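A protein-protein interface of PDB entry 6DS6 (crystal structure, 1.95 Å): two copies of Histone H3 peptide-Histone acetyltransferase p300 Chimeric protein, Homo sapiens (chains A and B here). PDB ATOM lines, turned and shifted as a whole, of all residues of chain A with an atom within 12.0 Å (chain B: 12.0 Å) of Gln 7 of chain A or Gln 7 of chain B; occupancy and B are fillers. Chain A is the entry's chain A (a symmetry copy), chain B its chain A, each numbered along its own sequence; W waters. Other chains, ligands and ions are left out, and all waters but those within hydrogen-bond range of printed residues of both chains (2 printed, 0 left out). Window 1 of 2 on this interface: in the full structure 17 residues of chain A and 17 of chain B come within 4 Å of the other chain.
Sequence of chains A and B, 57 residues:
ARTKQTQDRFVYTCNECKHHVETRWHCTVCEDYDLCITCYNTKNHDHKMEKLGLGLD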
ATOM      1  N   THR A   3      -8.615   1.670 -14.296  1.00  0.00           N
ATOM      2  CA  THR A   3      -9.522   0.813 -15.045  1.00  0.00           C
ATOM      3  C   THR A   3      -8.944   0.577 -16.440  1.00  0.00           C
ATOM      4  O   THR A   3      -8.008   1.252 -16.877  1.00  0.00           O
ATOM      5  CB  THR A   3     -10.923   1.412 -15.180  1.00  0.00           C
ATOM      6  OG1 THR A   3     -10.840   2.626 -15.927  1.00  0.00           O
ATOM      7  CG2 THR A   3     -11.570   1.683 -13.797  1.00  0.00           C
ATOM      8  N   LYS A   4      -9.513  -0.389 -17.146  1.00  0.00           N
ATOM      9  CA  LYS A   4      -9.097  -0.680 -18.512  1.00  0.00           C
ATOM     10  C   LYS A   4      -9.865   0.207 -19.482  1.00  0.00           C
ATOM     11  O   LYS A   4     -11.048   0.489 -19.285  1.00  0.00           O
ATOM     12  CB  LYS A   4      -9.324  -2.152 -18.864  1.00  0.00           C
ATOM     13  CG  LYS A   4      -8.476  -3.142 -18.087  1.00  0.00           C
ATOM     14  CD  LYS A   4      -7.040  -3.098 -18.533  1.00  0.00           C
ATOM     15  CE  LYS A   4      -6.266  -4.331 -18.088  1.00  0.00           C
ATOM     16  NZ  LYS A   4      -6.523  -5.563 -18.882  1.00  0.00           N
ATOM     17  N   GLN A   5      -9.179   0.668 -20.519  1.00  0.00           N
ATOM     18  CA  GLN A   5      -9.826   1.303 -21.652  1.00  0.00           C
ATOM     19  C   GLN A   5      -9.432   0.537 -22.906  1.00  0.00           C
ATOM     20  O   GLN A   5      -8.250   0.235 -23.108  1.00  0.00           O
ATOM     21  CB  GLN A   5      -9.432   2.768 -21.789  1.00  0.00           C
ATOM     22  CG  GLN A   5      -9.950   3.385 -23.062  1.00  0.00           C
ATOM     23  CD  GLN A   5      -9.484   4.809 -23.258  1.00  0.00           C
ATOM     24  OE1 GLN A   5      -8.509   5.069 -23.963  1.00  0.00           O
ATOM     25  NE2 GLN A   5     -10.192   5.740 -22.661  1.00  0.00           N
ATOM     26  N   THR A   6     -10.411   0.247 -23.747  1.00  0.00           N
ATOM     27  CA  THR A   6     -10.168  -0.390 -25.030  1.00  0.00           C
ATOM     28  C   THR A   6      -9.829   0.661 -26.081  1.00  0.00           C
ATOM     29  O   THR A   6     -10.408   1.748 -26.103  1.00  0.00           O
ATOM     30  CB  THR A   6     -11.396  -1.199 -25.442  1.00  0.00           C
ATOM     31  OG1 THR A   6     -11.515  -2.314 -24.562  1.00  0.00           O
ATOM     32  CG2 THR A   6     -11.265  -1.750 -26.901  1.00  0.00           C
ATOM     33  N   GLN A   7      -8.860   0.341 -26.932  1.00  0.00           N
ATOM     34  CA  GLN A   7      -8.462   1.226 -28.015  1.00  0.00           C
ATOM     35  C   GLN A   7      -7.845   0.375 -29.122  1.00  0.00           C
ATOM     36  O   GLN A   7      -7.728  -0.848 -28.991  1.00  0.00           O
ATOM     37  CB  GLN A   7      -7.496   2.288 -27.515  1.00  0.00           C
ATOM     38  CG  GLN A   7      -6.208   1.732 -26.950  1.00  0.00           C
ATOM     39  CD  GLN A   7      -5.373   2.808 -26.299  1.00  0.00           C
ATOM     40  OE1 GLN A   7      -5.899   3.724 -25.657  1.00  0.00           O
ATOM     41  NE2 GLN A   7      -4.069   2.706 -26.455  1.00  0.00           N
ATOM     42  N   ASP A   8      -7.471   1.014 -30.230  1.00  0.00           N
ATOM     43  CA  ASP A   8      -6.850   0.262 -31.312  1.00  0.00           C
ATOM     44  C   ASP A   8      -5.495   0.849 -31.689  1.00  0.00           C
ATOM     45  O   ASP A   8      -5.059   1.884 -31.172  1.00  0.00           O
ATOM     46  CB  ASP A   8      -7.778   0.142 -32.542  1.00  0.00           C
ATOM     47  CG  ASP A   8      -8.041   1.459 -33.264  1.00  0.00           C
ATOM     48  OD1 ASP A   8      -7.291   2.452 -33.129  1.00  0.00           O
ATOM     49  OD2 ASP A   8      -9.045   1.476 -34.005  1.00  0.00           O
ATOM     50  N   ARG A   9      -4.812   0.128 -32.572  1.00  0.00           N
ATOM     51  CA  ARG A   9      -3.525   0.549 -33.100  1.00  0.00           C
ATOM     52  C   ARG A   9      -3.343  -0.082 -34.475  1.00  0.00           C
ATOM     53  O   ARG A   9      -4.071  -0.994 -34.863  1.00  0.00           O
ATOM     54  CB  ARG A   9      -2.391   0.151 -32.164  1.00  0.00           C
ATOM     55  CG  ARG A   9      -2.168  -1.337 -32.089  1.00  0.00           C
ATOM     56  CD  ARG A   9      -0.688  -1.610 -31.988  1.00  0.00           C
ATOM     57  NE  ARG A   9      -0.394  -2.882 -31.346  1.00  0.00           N
ATOM     58  CZ  ARG A   9       0.766  -3.517 -31.470  1.00  0.00           C
ATOM     59  NH1 ARG A   9       1.734  -2.984 -32.213  1.00  0.00           N
ATOM     60  NH2 ARG A   9       0.958  -4.679 -30.852  1.00  0.00           N
ATOM     61  N   PHE A  10      -2.375   0.423 -35.222  1.00  0.00           N
ATOM     62  CA  PHE A  10      -2.069  -0.143 -36.524  1.00  0.00           C
ATOM     63  C   PHE A  10      -0.989  -1.198 -36.389  1.00  0.00           C
ATOM     64  O   PHE A  10      -0.016  -1.011 -35.663  1.00  0.00           O
ATOM     65  CB  PHE A  10      -1.613   0.935 -37.496  1.00  0.00           C
ATOM     66  CG  PHE A  10      -2.723   1.795 -37.996  1.00  0.00           C
ATOM     67  CD1 PHE A  10      -3.604   1.324 -38.946  1.00  0.00           C
ATOM     68  CD2 PHE A  10      -2.886   3.079 -37.514  1.00  0.00           C
ATOM     69  CE1 PHE A  10      -4.629   2.123 -39.417  1.00  0.00           C
ATOM     70  CE2 PHE A  10      -3.906   3.876 -37.981  1.00  0.00           C
ATOM     71  CZ  PHE A  10      -4.778   3.397 -38.933  1.00  0.00           C
ATOM     72  N   VAL A  11      -1.178  -2.315 -37.087  1.00  0.00           N
ATOM     73  CA  VAL A  11      -0.190  -3.378 -37.175  1.00  0.00           C
ATOM     74  C   VAL A  11       0.125  -3.559 -38.660  1.00  0.00           C
ATOM     75  O   VAL A  11      -0.789  -3.560 -39.493  1.00  0.00           O
ATOM     76  CB  VAL A  11      -0.702  -4.683 -36.538  1.00  0.00           C
ATOM     77  CG1 VAL A  11      -0.895  -4.519 -34.987  1.00  0.00           C
ATOM     78  CG2 VAL A  11      -2.020  -5.063 -37.148  1.00  0.00           C
ATOM     79  N   TYR A  12       1.409  -3.656 -38.993  1.00  0.00           N
ATOM     80  CA  TYR A  12       1.864  -3.657 -40.384  1.00  0.00           C
ATOM     81  C   TYR A  12       2.491  -4.992 -40.765  1.00  0.00           C
ATOM     82  O   TYR A  12       3.161  -5.632 -39.949  1.00  0.00           O
ATOM     83  CB  TYR A  12       2.885  -2.528 -40.635  1.00  0.00           C
ATOM     84  CG  TYR A  12       2.328  -1.141 -40.410  1.00  0.00           C
ATOM     85  CD1 TYR A  12       1.840  -0.385 -41.462  1.00  0.00           C
ATOM     86  CD2 TYR A  12       2.271  -0.594 -39.129  1.00  0.00           C
ATOM     87  CE1 TYR A  12       1.326   0.880 -41.252  1.00  0.00           C
ATOM     88  CE2 TYR A  12       1.760   0.666 -38.911  1.00  0.00           C
ATOM     89  CZ  TYR A  12       1.280   1.396 -39.974  1.00  0.00           C
ATOM     90  OH  TYR A  12       0.768   2.651 -39.756  1.00  0.00           O
ATOM     91  N   HIS A  20       5.279  -9.780 -40.339  1.00  0.00           N
ATOM     92  CA  HIS A  20       5.091  -8.621 -39.475  1.00  0.00           C
ATOM     93  C   HIS A  20       6.302  -7.701 -39.559  1.00  0.00           C
ATOM     94  O   HIS A  20       7.449  -8.157 -39.518  1.00  0.00           O
ATOM     95  CB  HIS A  20       4.872  -9.103 -38.030  1.00  0.00           C
ATOM     96  CG  HIS A  20       4.795  -8.011 -37.001  1.00  0.00           C
ATOM     97  ND1 HIS A  20       3.725  -7.145 -36.902  1.00  0.00           N
ATOM     98  CD2 HIS A  20       5.637  -7.678 -35.993  1.00  0.00           C
ATOM     99  CE1 HIS A  20       3.925  -6.311 -35.896  1.00  0.00           C
ATOM    100  NE2 HIS A  20       5.080  -6.612 -35.329  1.00  0.00           N
ATOM    101  N   GLU A  22       7.831  -3.769 -38.103  1.00  0.00           N
ATOM    102  CA  GLU A  22       7.725  -2.504 -37.399  1.00  0.00           C
ATOM    103  C   GLU A  22       8.543  -1.418 -38.074  1.00  0.00           C
ATOM    104  O   GLU A  22       8.012  -0.345 -38.384  1.00  0.00           O
ATOM    105  CB  GLU A  22       8.135  -2.661 -35.925  1.00  0.00           C
ATOM    106  CG  GLU A  22       6.950  -3.040 -35.041  1.00  0.00           C
ATOM    107  CD  GLU A  22       7.343  -3.790 -33.787  1.00  0.00           C
ATOM    108  OE1 GLU A  22       8.555  -3.861 -33.477  1.00  0.00           O
ATOM    109  OE2 GLU A  22       6.431  -4.321 -33.119  1.00  0.00           O
ATOM    110  N   THR B   3      -3.487  -3.056 -40.840  1.00  0.00           N
ATOM    111  CA  THR B   3      -4.815  -3.345 -40.319  1.00  0.00           C
ATOM    112  C   THR B   3      -4.898  -2.854 -38.873  1.00  0.00           C
ATOM    113  O   THR B   3      -3.890  -2.533 -38.238  1.00  0.00           O
ATOM    114  CB  THR B   3      -5.154  -4.835 -40.361  1.00  0.00           C
ATOM    115  OG1 THR B   3      -4.248  -5.542 -39.513  1.00  0.00           O
ATOM    116  CG2 THR B   3      -5.083  -5.402 -41.803  1.00  0.00           C
ATOM    117  N   LYS B   4      -6.114  -2.803 -38.350  1.00  0.00           N
ATOM    118  CA  LYS B   4      -6.329  -2.410 -36.962  1.00  0.00           C
ATOM    119  C   LYS B   4      -6.209  -3.629 -36.058  1.00  0.00           C
ATOM    120  O   LYS B   4      -6.625  -4.731 -36.419  1.00  0.00           O
ATOM    121  CB  LYS B   4      -7.701  -1.757 -36.773  1.00  0.00           C
ATOM    122  CG  LYS B   4      -7.890  -0.430 -37.483  1.00  0.00           C
ATOM    123  CD  LYS B   4      -7.106   0.664 -36.811  1.00  0.00           C
ATOM    124  CE  LYS B   4      -7.586   2.049 -37.226  1.00  0.00           C
ATOM    125  NZ  LYS B   4      -8.852   2.499 -36.587  1.00  0.00           N
ATOM    126  N   GLN B   5      -5.612  -3.432 -34.891  1.00  0.00           N
ATOM    127  CA  GLN B   5      -5.651  -4.419 -33.828  1.00  0.00           C
ATOM    128  C   GLN B   5      -6.244  -3.754 -32.594  1.00  0.00           C
ATOM    129  O   GLN B   5      -5.845  -2.643 -32.231  1.00  0.00           O
ATOM    130  CB  GLN B   5      -4.269  -4.973 -33.509  1.00  0.00           C
ATOM    131  CG  GLN B   5      -4.271  -5.857 -32.290  1.00  0.00           C
ATOM    132  CD  GLN B   5      -2.890  -6.334 -31.905  1.00  0.00           C
ATOM    133  OE1 GLN B   5      -2.237  -5.759 -31.035  1.00  0.00           O
ATOM    134  NE2 GLN B   5      -2.448  -7.402 -32.530  1.00  0.00           N
ATOM    135  N   THR B   6      -7.171  -4.442 -31.947  1.00  0.00           N
ATOM    136  CA  THR B   6      -7.751  -3.977 -30.698  1.00  0.00           C
ATOM    137  C   THR B   6      -6.879  -4.408 -29.524  1.00  0.00           C
ATOM    138  O   THR B   6      -6.337  -5.514 -29.506  1.00  0.00           O
ATOM    139  CB  THR B   6      -9.170  -4.525 -30.556  1.00  0.00           C
ATOM    140  OG1 THR B   6      -9.994  -3.894 -31.533  1.00  0.00           O
ATOM    141  CG2 THR B   6      -9.771  -4.216 -29.146  1.00  0.00           C
ATOM    142  N   GLN B   7      -6.720  -3.509 -28.559  1.00  0.00           N
ATOM    143  CA  GLN B   7      -5.954  -3.797 -27.356  1.00  0.00           C
ATOM    144  C   GLN B   7      -6.464  -2.892 -26.239  1.00  0.00           C
ATOM    145  O   GLN B   7      -7.361  -2.069 -26.450  1.00  0.00           O
ATOM    146  CB  GLN B   7      -4.466  -3.602 -27.607  1.00  0.00           C
ATOM    147  CG  GLN B   7      -4.089  -2.192 -28.002  1.00  0.00           C
ATOM    148  CD  GLN B   7      -2.642  -2.098 -28.421  1.00  0.00           C
ATOM    149  OE1 GLN B   7      -2.101  -3.007 -29.061  1.00  0.00           O
ATOM    150  NE2 GLN B   7      -2.005  -1.000 -28.066  1.00  0.00           N
ATOM    151  N   ASP B   8      -5.913  -3.057 -25.037  1.00  0.00           N
ATOM    152  CA  ASP B   8      -6.338  -2.204 -23.934  1.00  0.00           C
ATOM    153  C   ASP B   8      -5.152  -1.489 -23.299  1.00  0.00           C
ATOM    154  O   ASP B   8      -3.986  -1.703 -23.652  1.00  0.00           O
ATOM    155  CB  ASP B   8      -7.161  -2.982 -22.883  1.00  0.00           C
ATOM    156  CG  ASP B   8      -6.366  -4.026 -22.107  1.00  0.00           C
ATOM    157  OD1 ASP B   8      -5.117  -3.994 -22.038  1.00  0.00           O
ATOM    158  OD2 ASP B   8      -7.044  -4.905 -21.537  1.00  0.00           O
ATOM    159  N   ARG B   9      -5.484  -0.588 -22.380  1.00  0.00           N
ATOM    160  CA  ARG B   9      -4.495   0.159 -21.619  1.00  0.00           C
ATOM    161  C   ARG B   9      -5.120   0.563 -20.290  1.00  0.00           C
ATOM    162  O   ARG B   9      -6.332   0.480 -20.100  1.00  0.00           O
ATOM    163  CB  ARG B   9      -4.019   1.382 -22.391  1.00  0.00           C
ATOM    164  CG  ARG B   9      -5.077   2.441 -22.552  1.00  0.00           C
ATOM    165  CD  ARG B   9      -4.436   3.802 -22.436  1.00  0.00           C
ATOM    166  NE  ARG B   9      -5.190   4.838 -23.125  1.00  0.00           N
ATOM    167  CZ  ARG B   9      -5.059   6.135 -22.870  1.00  0.00           C
ATOM    168  NH1 ARG B   9      -4.197   6.541 -21.940  1.00  0.00           N
ATOM    169  NH2 ARG B   9      -5.787   7.022 -23.543  1.00  0.00           N
ATOM    170  N   PHE B  10      -4.279   0.984 -19.359  1.00  0.00           N
ATOM    171  CA  PHE B  10      -4.770   1.457 -18.076  1.00  0.00           C
ATOM    172  C   PHE B  10      -4.981   2.956 -18.122  1.00  0.00           C
ATOM    173  O   PHE B  10      -4.159   3.690 -18.665  1.00  0.00           O
ATOM    174  CB  PHE B  10      -3.796   1.111 -16.957  1.00  0.00           C
ATOM    175  CG  PHE B  10      -3.817  -0.329 -16.573  1.00  0.00           C
ATOM    176  CD1 PHE B  10      -4.852  -0.840 -15.818  1.00  0.00           C
ATOM    177  CD2 PHE B  10      -2.799  -1.174 -16.968  1.00  0.00           C
ATOM    178  CE1 PHE B  10      -4.869  -2.173 -15.453  1.00  0.00           C
ATOM    179  CE2 PHE B  10      -2.815  -2.502 -16.606  1.00  0.00           C
ATOM    180  CZ  PHE B  10      -3.850  -3.002 -15.849  1.00  0.00           C
ATOM    181  N   VAL B  11      -6.100   3.403 -17.557  1.00  0.00           N
ATOM    182  CA  VAL B  11      -6.407   4.815 -17.400  1.00  0.00           C
ATOM    183  C   VAL B  11      -6.610   5.053 -15.903  1.00  0.00           C
ATOM    184  O   VAL B  11      -7.266   4.250 -15.230  1.00  0.00           O
ATOM    185  CB  VAL B  11      -7.647   5.222 -18.215  1.00  0.00           C
ATOM    186  CG1 VAL B  11      -7.377   5.097 -19.759  1.00  0.00           C
ATOM    187  CG2 VAL B  11      -8.804   4.333 -17.857  1.00  0.00           C
ATOM    188  N   TYR B  12      -6.008   6.117 -15.378  1.00  0.00           N
ATOM    189  CA  TYR B  12      -5.972   6.370 -13.937  1.00  0.00           C
ATOM    190  C   TYR B  12      -6.751   7.627 -13.571  1.00  0.00           C
ATOM    191  O   TYR B  12      -6.753   8.610 -14.319  1.00  0.00           O
ATOM    192  CB  TYR B  12      -4.521   6.509 -13.434  1.00  0.00           C
ATOM    193  CG  TYR B  12      -3.685   5.265 -13.631  1.00  0.00           C
ATOM    194  CD1 TYR B  12      -3.524   4.341 -12.612  1.00  0.00           C
ATOM    195  CD2 TYR B  12      -3.073   5.003 -14.855  1.00  0.00           C
ATOM    196  CE1 TYR B  12      -2.765   3.202 -12.797  1.00  0.00           C
ATOM    197  CE2 TYR B  12      -2.314   3.869 -15.048  1.00  0.00           C
ATOM    198  CZ  TYR B  12      -2.171   2.967 -14.020  1.00  0.00           C
ATOM    199  OH  TYR B  12      -1.417   1.835 -14.213  1.00  0.00           O
ATOM    200  N   HIS B  20      -8.948  12.719 -13.937  1.00  0.00           N
ATOM    201  CA  HIS B  20      -7.983  11.958 -14.722  1.00  0.00           C
ATOM    202  C   HIS B  20      -6.564  12.386 -14.370  1.00  0.00           C
ATOM    203  O   HIS B  20      -6.270  13.581 -14.264  1.00  0.00           O
ATOM    204  CB  HIS B  20      -8.264  12.183 -16.218  1.00  0.00           C
ATOM    205  CG  HIS B  20      -7.264  11.564 -17.153  1.00  0.00           C
ATOM    206  ND1 HIS B  20      -7.162  10.202 -17.350  1.00  0.00           N
ATOM    207  CD2 HIS B  20      -6.354  12.130 -17.983  1.00  0.00           C
ATOM    208  CE1 HIS B  20      -6.215   9.957 -18.240  1.00  0.00           C
ATOM    209  NE2 HIS B  20      -5.707  11.109 -18.638  1.00  0.00           N
ATOM    210  N   GLU B  22      -2.292  11.428 -15.235  1.00  0.00           N
ATOM    211  CA  GLU B  22      -1.221  10.658 -15.840  1.00  0.00           C
ATOM    212  C   GLU B  22       0.013  10.624 -14.956  1.00  0.00           C
ATOM    213  O   GLU B  22       0.524   9.541 -14.649  1.00  0.00           O
ATOM    214  CB  GLU B  22      -0.877  11.201 -17.238  1.00  0.00           C
ATOM    215  CG  GLU B  22      -1.718  10.542 -18.328  1.00  0.00           C
ATOM    216  CD  GLU B  22      -1.896  11.403 -19.560  1.00  0.00           C
ATOM    217  OE1 GLU B  22      -1.212  12.445 -19.677  1.00  0.00           O
ATOM    218  OE2 GLU B  22      -2.738  11.034 -20.407  1.00  0.00           O
HETATM  219  O   HOH W   1      -9.706   4.937 -14.468  1.00  0.00           O
HETATM  220  O   HOH W   2      -1.507  -5.866 -40.577  1.00  0.00           O
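N of Gln 7 of chain B sits at hydrogen-bond distance from O of Gln 7 of chain A, 2.9 Å away.
O of Arg 9 of chain B lies within hydrogen-bond range of N of Gln 5 of chain A (2.9 Å).
The guanidinium group (NE) of Arg 9 of chain B sits at hydrogen-bond distance from the side-chain amide oxygen (OE1) of Gln 7 of chain A (2.9 Å).
OD2 of Asp 8 of chain B lies within salt-bridge range of NZ of Lys 4 of chain A.
The backbone NH of Val 11 of chain B lies within hydrogen-bond range of the backbone carbonyl oxygen of Thr 3 of chain A (3.0 Å).
The backbone NH of Gln 5 of chain B lies within hydrogen-bond range of the backbone carbonyl oxygen of Arg 9 of chain A.
O of Thr 3 of chain B lies within hydrogen-bond range of N of Val 11 of chain A (3.0 Å).
NZ of Lys 4 of chain B is in salt-bridge range of OD2 of Asp 8 of chain A (2.8 Å).
OE1 of Gln 7 of chain B is in hydrogen-bond range of NE of Arg 9 of chain A.
The side-chain amide oxygen (OE1) of Gln 5 of chain A lies close to the side-chain amide oxygen (OE1) of Gln 7 of chain A, at 3.4 Å.
OE1 of Gln 5 of chain B lies close to OE1 of Gln 7 of chain B (3.4 Å).
Among the printed residues, merely in contact across the chains: Gln 5 of chain A with Asp 8 of chain B, Asp 8 of chain A with Gln 5 of chain B, Arg 9 of chain A with Lys 4 of chain B, Lys 4 of chain A with Arg 9 of chain B, Thr 3 of chain A with Phe 10 of chain B, Phe 10 of chain A with Thr 3 of chain B, Phe 10 of chain A with Lys 4 of chain B, Lys 4 of chain A with Phe 10 of chain B, Gln 7 of chain A with Thr 6 of chain B, Thr 6 of chain A with Gln 7 of chain B, Thr 6 of chain A with Thr 6 of chain B, Gln 5 of chain A with Val 11 of chain B, Val 11 of chain A with Gln 5 of chain B, Arg 9 of chain A with Thr 3 of chain B and Thr 3 of chain A with Arg 9 of chain B.
Thr 6 of chain A touches just these residues of chain B: Thr 6 (3.7 Å) and Gln 7 (3.6 Å).
Of chain B, only Lys 4 and Gln 5 come within 4 Å of Asp 8 of chain A.
Arg 9 of chain A touches just these residues of chain B: Thr 3, Lys 4, Gln 5 and Gln 7.
Printed residues of chain A within 4 Å of Lys 4 of chain B: Asp 8, Arg 9 and Phe 10.
Of chain A, only Thr 6 and Gln 7 come within 4 Å of Thr 6 of chain B.
Of the printed residues of chain A, Asp 8 of chain B touches Lys 4 and Gln 5.
Arg 9 of chain B touches just these residues of chain A: Thr 3 (3.7 Å), Lys 4 (3.4 Å), Gln 5 (2.9 Å) and Gln 7 (2.9 Å).
Of the printed residues of chain A, Phe 10 of chain B touches Thr 3 and Lys 4.
His 20 of chain B touches none of the printed residues of chain A.
Glu 22 of chain B touches none of the printed residues of chain A.
The nearest residue of chain B that does not touch Gln 7 of chain A is Gln 5 of chain B (4.2 Å).
The nearest residue of chain A that does not touch Gln 7 of chain B is Gln 5 of chain A (4.2 Å).
The nearest printed residue of chain A that does not touch Thr 3 of chain B is Tyr 12 of chain A (5.3 Å).
Hydrophobic or aromatic side chains of chain A within 4 Å of the printed part of chain B: Phe 10 and Val 11.
Of the 12 printed residues of chain B, 9 touch a printed residue of chain A.
Printed residues of chain B that touch a printed residue of chain A: Thr 3, Lys 4, Gln 5, Thr 6, Gln 7, Asp 8, Arg 9, Phe 10 and Val 11.
Hydrophobic or aromatic side chains of chain B within 4 Å of the printed part of chain A: Phe 10 and Val 11.
Among the printed residues, 24 pairs touch across the chains.
Among the printed residues, Asp or Glu carboxylates within 4 Å of a Lys or Arg side-chain nitrogen of the other chain: Lys 4 of chain A with Asp 8 of chain B and Asp 8 of chain A with Lys 4 of chain B.
Thr 3 of chain A touches Phe 10 of chain B, and with the chains exchanged Phe 10 of chain A touches Thr 3 of chain B.
Lys 4 of chain A touches Phe 10 of chain B, and with the chains exchanged Phe 10 of chain A touches Lys 4 of chain B.
Gln 5 of chain A touches Arg 9 of chain B, and with the chains exchanged Arg 9 of chain A touches Gln 5 of chain B.
Gln 7 of chain A touches its own counterpart, Gln 7 of chain B.
Water W2 lies within hydrogen-bond range of the backbone carbonyl oxygen (O) of Val 11 of chain A (2.6 Å) and the side-chain hydroxyl (OG1) of Thr 3 of chain B (3.0 Å).
Water W1 lies within hydrogen-bond range of the backbone carbonyl oxygen (O) of Val 11 of chain B (2.6 Å) and the side-chain hydroxyl (OG1) of Thr 3 of chain A (3.0 Å).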
